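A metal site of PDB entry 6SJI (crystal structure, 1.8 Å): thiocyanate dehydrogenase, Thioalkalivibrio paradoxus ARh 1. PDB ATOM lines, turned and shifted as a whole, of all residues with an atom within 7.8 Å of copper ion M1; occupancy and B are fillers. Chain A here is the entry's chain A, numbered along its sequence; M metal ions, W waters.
O of Ser 250 sits at hydrogen-bond distance from N of Asp 236, at 3.0 Å.
Of the 18 residues printed, 3 come within 4 Å of copper ion M1.
Copper ion M1 is bound by NE2 of His 128.
NE2 of His 303 binds copper ion M1 (1.9 Å).
Copper ion M1 is bound by the side-chain carboxylate (OD2) of Asp 236.
Copper ion M1 is bound by OD1 of Asp 236.
Copper ion M1 has four donor atoms within binding distance.
Slightly farther from copper ion M1 lies water W1 (2.7 Å).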
ATOM      1  N   HIS A  57     -21.157  12.036 -17.745  1.00  0.00           N
ATOM      2  CA  HIS A  57     -21.256  11.149 -16.614  1.00  0.00           C
ATOM      3  C   HIS A  57     -22.599  11.243 -15.857  1.00  0.00           C
ATOM      4  O   HIS A  57     -23.554  10.527 -16.207  1.00  0.00           O
ATOM      5  CB  HIS A  57     -20.102  11.277 -15.637  1.00  0.00           C
ATOM      6  CG  HIS A  57     -20.005  10.098 -14.715  1.00  0.00           C
ATOM      7  ND1 HIS A  57     -19.278  10.110 -13.547  1.00  0.00           N
ATOM      8  CD2 HIS A  57     -20.518   8.854 -14.834  1.00  0.00           C
ATOM      9  CE1 HIS A  57     -19.334   8.911 -12.991  1.00  0.00           C
ATOM     10  NE2 HIS A  57     -20.094   8.137 -13.750  1.00  0.00           N
ATOM     11  N   HIS A  58     -22.690  12.104 -14.824  1.00  0.00           N
ATOM     12  CA  HIS A  58     -23.949  12.230 -14.100  1.00  0.00           C
ATOM     13  C   HIS A  58     -24.698  13.468 -14.496  1.00  0.00           C
ATOM     14  O   HIS A  58     -24.128  14.368 -15.145  1.00  0.00           O
ATOM     15  CB  HIS A  58     -23.720  12.135 -12.596  1.00  0.00           C
ATOM     16  CG  HIS A  58     -23.346  10.762 -12.150  1.00  0.00           C
ATOM     17  ND1 HIS A  58     -24.230   9.711 -12.251  1.00  0.00           N
ATOM     18  CD2 HIS A  58     -22.198  10.255 -11.653  1.00  0.00           C
ATOM     19  CE1 HIS A  58     -23.637   8.600 -11.814  1.00  0.00           C
ATOM     20  NE2 HIS A  58     -22.395   8.911 -11.448  1.00  0.00           N
ATOM     21  N   VAL A 127     -18.380  13.145 -10.153  1.00  0.00           N
ATOM     22  CA  VAL A 127     -19.310  12.073  -9.827  1.00  0.00           C
ATOM     23  C   VAL A 127     -20.710  12.627  -9.721  1.00  0.00           C
ATOM     24  O   VAL A 127     -21.093  13.327 -10.653  1.00  0.00           O
ATOM     25  CB  VAL A 127     -18.814  11.211  -8.616  1.00  0.00           C
ATOM     26  CG1 VAL A 127     -19.636   9.920  -8.580  1.00  0.00           C
ATOM     27  CG2 VAL A 127     -17.316  10.857  -8.871  1.00  0.00           C
ATOM     28  N   HIS A 128     -21.493  12.374  -8.663  1.00  0.00           N
ATOM     29  CA  HIS A 128     -22.957  12.610  -8.776  1.00  0.00           C
ATOM     30  C   HIS A 128     -23.303  14.069  -8.812  1.00  0.00           C
ATOM     31  O   HIS A 128     -22.653  14.843  -8.145  1.00  0.00           O
ATOM     32  CB  HIS A 128     -23.735  11.925  -7.673  1.00  0.00           C
ATOM     33  CG  HIS A 128     -23.714  10.438  -7.787  1.00  0.00           C
ATOM     34  ND1 HIS A 128     -24.572   9.722  -8.613  1.00  0.00           N
ATOM     35  CD2 HIS A 128     -22.942   9.528  -7.139  1.00  0.00           C
ATOM     36  CE1 HIS A 128     -24.298   8.421  -8.476  1.00  0.00           C
ATOM     37  NE2 HIS A 128     -23.298   8.286  -7.620  1.00  0.00           N
ATOM     38  N   GLU A 210     -12.313   6.989 -10.489  1.00  0.00           N
ATOM     39  CA  GLU A 210     -13.336   6.741  -9.486  1.00  0.00           C
ATOM     40  C   GLU A 210     -13.335   5.224  -9.205  1.00  0.00           C
ATOM     41  O   GLU A 210     -13.294   4.435 -10.168  1.00  0.00           O
ATOM     42  CB  GLU A 210     -14.697   7.165 -10.062  1.00  0.00           C
ATOM     43  CG  GLU A 210     -15.923   6.804  -9.231  1.00  0.00           C
ATOM     44  CD  GLU A 210     -17.245   6.933 -10.003  1.00  0.00           C
ATOM     45  OE1 GLU A 210     -17.261   7.367 -11.187  1.00  0.00           O
ATOM     46  OE2 GLU A 210     -18.321   6.670  -9.413  1.00  0.00           O
ATOM     47  N   ASN A 235     -15.601  10.208  -1.766  1.00  0.00           N
ATOM     48  CA  ASN A 235     -16.919  10.896  -1.714  1.00  0.00           C
ATOM     49  C   ASN A 235     -17.709  10.551  -2.986  1.00  0.00           C
ATOM     50  O   ASN A 235     -17.105  10.392  -4.069  1.00  0.00           O
ATOM     51  CB  ASN A 235     -16.721  12.421  -1.543  1.00  0.00           C
ATOM     52  CG  ASN A 235     -17.978  13.208  -1.785  1.00  0.00           C
ATOM     53  OD1 ASN A 235     -18.040  14.036  -2.731  1.00  0.00           O
ATOM     54  ND2 ASN A 235     -19.024  12.958  -0.964  1.00  0.00           N
ATOM     55  N   ASP A 236     -19.028  10.438  -2.901  1.00  0.00           N
ATOM     56  CA  ASP A 236     -19.812   9.963  -4.031  1.00  0.00           C
ATOM     57  C   ASP A 236     -20.808  11.053  -4.423  1.00  0.00           C
ATOM     58  O   ASP A 236     -20.870  11.454  -5.537  1.00  0.00           O
ATOM     59  CB  ASP A 236     -20.553   8.661  -3.627  1.00  0.00           C
ATOM     60  CG  ASP A 236     -21.328   8.063  -4.757  1.00  0.00           C
ATOM     61  OD1 ASP A 236     -20.696   7.736  -5.778  1.00  0.00           O
ATOM     62  OD2 ASP A 236     -22.580   7.927  -4.645  1.00  0.00           O
ATOM     63  N   ALA A 237     -21.581  11.563  -3.449  1.00  0.00           N
ATOM     64  CA  ALA A 237     -22.699  12.435  -3.789  1.00  0.00           C
ATOM     65  C   ALA A 237     -22.943  13.429  -2.637  1.00  0.00           C
ATOM     66  O   ALA A 237     -22.481  13.166  -1.469  1.00  0.00           O
ATOM     67  CB  ALA A 237     -23.940  11.581  -4.072  1.00  0.00           C
ATOM     68  N   SER A 250     -22.071  11.483   0.985  1.00  0.00           N
ATOM     69  CA  SER A 250     -21.831  10.030   1.241  1.00  0.00           C
ATOM     70  C   SER A 250     -20.354   9.809   0.988  1.00  0.00           C
ATOM     71  O   SER A 250     -19.823  10.383   0.011  1.00  0.00           O
ATOM     72  CB  SER A 250     -22.664   9.127   0.292  1.00  0.00           C
ATOM     73  OG  SER A 250     -22.622   9.750  -0.979  1.00  0.00           O
ATOM     74  N   ARG A 252     -17.773   6.668   0.483  1.00  0.00           N
ATOM     75  CA  ARG A 252     -17.735   5.219   0.252  1.00  0.00           C
ATOM     76  C   ARG A 252     -16.785   4.467   1.176  1.00  0.00           C
ATOM     77  O   ARG A 252     -17.185   3.459   1.832  1.00  0.00           O
ATOM     78  CB  ARG A 252     -17.426   4.928  -1.254  1.00  0.00           C
ATOM     79  CG  ARG A 252     -18.629   5.400  -2.115  1.00  0.00           C
ATOM     80  CD  ARG A 252     -18.286   5.148  -3.598  1.00  0.00           C
ATOM     81  NE  ARG A 252     -17.933   3.755  -3.855  1.00  0.00           N
ATOM     82  CZ  ARG A 252     -17.399   3.350  -5.005  1.00  0.00           C
ATOM     83  NH1 ARG A 252     -17.182   4.236  -5.987  1.00  0.00           N
ATOM     84  NH2 ARG A 252     -17.036   2.064  -5.136  1.00  0.00           N
ATOM     85  N   GLY A 302     -19.880   1.805   1.976  1.00  0.00           N
ATOM     86  CA  GLY A 302     -21.266   1.959   1.555  1.00  0.00           C
ATOM     87  C   GLY A 302     -21.340   2.800   0.283  1.00  0.00           C
ATOM     88  O   GLY A 302     -20.319   3.301  -0.165  1.00  0.00           O
ATOM     89  N   HIS A 303     -22.548   2.975  -0.304  1.00  0.00           N
ATOM     90  CA  HIS A 303     -22.585   3.765  -1.538  1.00  0.00           C
ATOM     91  C   HIS A 303     -23.888   4.577  -1.653  1.00  0.00           C
ATOM     92  O   HIS A 303     -23.906   5.789  -1.338  1.00  0.00           O
ATOM     93  CB  HIS A 303     -22.314   2.866  -2.793  1.00  0.00           C
ATOM     94  CG  HIS A 303     -22.138   3.636  -4.083  1.00  0.00           C
ATOM     95  ND1 HIS A 303     -21.297   3.207  -5.101  1.00  0.00           N
ATOM     96  CD2 HIS A 303     -22.733   4.771  -4.548  1.00  0.00           C
ATOM     97  CE1 HIS A 303     -21.362   4.056  -6.125  1.00  0.00           C
ATOM     98  NE2 HIS A 303     -22.209   5.040  -5.808  1.00  0.00           N
ATOM     99  N   GLN A 304     -24.966   3.952  -2.180  1.00  0.00           N
ATOM    100  CA  GLN A 304     -26.239   4.727  -2.413  1.00  0.00           C
ATOM    101  C   GLN A 304     -26.681   5.408  -1.120  1.00  0.00           C
ATOM    102  O   GLN A 304     -26.631   4.794  -0.046  1.00  0.00           O
ATOM    103  CB  GLN A 304     -27.382   3.804  -2.859  1.00  0.00           C
ATOM    104  CG  GLN A 304     -28.751   4.520  -3.036  1.00  0.00           C
ATOM    105  CD  GLN A 304     -28.697   5.760  -3.943  1.00  0.00           C
ATOM    106  OE1 GLN A 304     -29.489   6.735  -3.783  1.00  0.00           O
ATOM    107  NE2 GLN A 304     -27.805   5.730  -4.927  1.00  0.00           N
ATOM    108  N   ALA A 305     -27.111   6.669  -1.222  1.00  0.00           N
ATOM    109  CA  ALA A 305     -27.566   7.386  -0.049  1.00  0.00           C
ATOM    110  C   ALA A 305     -28.735   8.230  -0.545  1.00  0.00           C
ATOM    111  O   ALA A 305     -28.666   8.795  -1.663  1.00  0.00           O
ATOM    112  CB  ALA A 305     -26.416   8.253   0.524  1.00  0.00           C
ATOM    113  N   PHE A 358     -26.505   0.217  -6.214  1.00  0.00           N
ATOM    114  CA  PHE A 358     -26.026   1.581  -6.185  1.00  0.00           C
ATOM    115  C   PHE A 358     -26.995   2.680  -6.645  1.00  0.00           C
ATOM    116  O   PHE A 358     -26.580   3.826  -6.606  1.00  0.00           O
ATOM    117  CB  PHE A 358     -24.539   1.792  -6.734  1.00  0.00           C
ATOM    118  CG  PHE A 358     -24.223   1.131  -8.061  1.00  0.00           C
ATOM    119  CD1 PHE A 358     -23.236   0.126  -8.139  1.00  0.00           C
ATOM    120  CD2 PHE A 358     -24.867   1.523  -9.257  1.00  0.00           C
ATOM    121  CE1 PHE A 358     -22.934  -0.477  -9.379  1.00  0.00           C
ATOM    122  CE2 PHE A 358     -24.572   0.925 -10.503  1.00  0.00           C
ATOM    123  CZ  PHE A 358     -23.598  -0.067 -10.558  1.00  0.00           C
ATOM    124  N   HIS A 359     -28.240   2.351  -7.067  1.00  0.00           N
ATOM    125  CA  HIS A 359     -29.190   3.425  -7.500  1.00  0.00           C
ATOM    126  C   HIS A 359     -30.593   3.147  -6.954  1.00  0.00           C
ATOM    127  O   HIS A 359     -30.940   1.959  -6.759  1.00  0.00           O
ATOM    128  CB  HIS A 359     -29.220   3.529  -9.009  1.00  0.00           C
ATOM    129  CG  HIS A 359     -27.911   3.938  -9.622  1.00  0.00           C
ATOM    130  ND1 HIS A 359     -27.321   5.171  -9.399  1.00  0.00           N
ATOM    131  CD2 HIS A 359     -27.071   3.262 -10.446  1.00  0.00           C
ATOM    132  CE1 HIS A 359     -26.184   5.237 -10.060  1.00  0.00           C
ATOM    133  NE2 HIS A 359     -26.000   4.090 -10.703  1.00  0.00           N
ATOM    134  N   HIS A 450     -24.780   6.259 -17.198  1.00  0.00           N
ATOM    135  CA  HIS A 450     -24.690   6.025 -15.761  1.00  0.00           C
ATOM    136  C   HIS A 450     -25.591   6.993 -15.038  1.00  0.00           C
ATOM    137  O   HIS A 450     -25.429   7.201 -13.827  1.00  0.00           O
ATOM    138  CB  HIS A 450     -23.253   6.213 -15.235  1.00  0.00           C
ATOM    139  CG  HIS A 450     -22.360   5.018 -15.506  1.00  0.00           C
ATOM    140  ND1 HIS A 450     -21.127   4.863 -14.915  1.00  0.00           N
ATOM    141  CD2 HIS A 450     -22.532   3.941 -16.311  1.00  0.00           C
ATOM    142  CE1 HIS A 450     -20.559   3.742 -15.345  1.00  0.00           C
ATOM    143  NE2 HIS A 450     -21.390   3.167 -16.197  1.00  0.00           N
ATOM    144  N   THR A 470     -29.604   9.153  -5.680  1.00  0.00           N
ATOM    145  CA  THR A 470     -28.871   8.984  -6.978  1.00  0.00           C
ATOM    146  C   THR A 470     -29.178   7.654  -7.679  1.00  0.00           C
ATOM    147  O   THR A 470     -28.617   7.350  -8.754  1.00  0.00           O
ATOM    148  CB  THR A 470     -27.342   9.150  -6.813  1.00  0.00           C
ATOM    149  OG1 THR A 470     -26.822   8.101  -5.974  1.00  0.00           O
ATOM    150  CG2 THR A 470     -26.994  10.495  -6.253  1.00  0.00           C
ATOM    151  OXT THR A 470     -29.999   6.844  -7.218  1.00  0.00           O
HETATM  152 CU    CU M   1     -22.739   6.676  -6.720  1.00  0.00          CU
HETATM  153 CU    CU M   2     -20.240   6.218 -13.883  1.00  0.00          CU
HETATM  154  O   HOH W   1     -23.093   5.247  -8.925  1.00  0.00           O
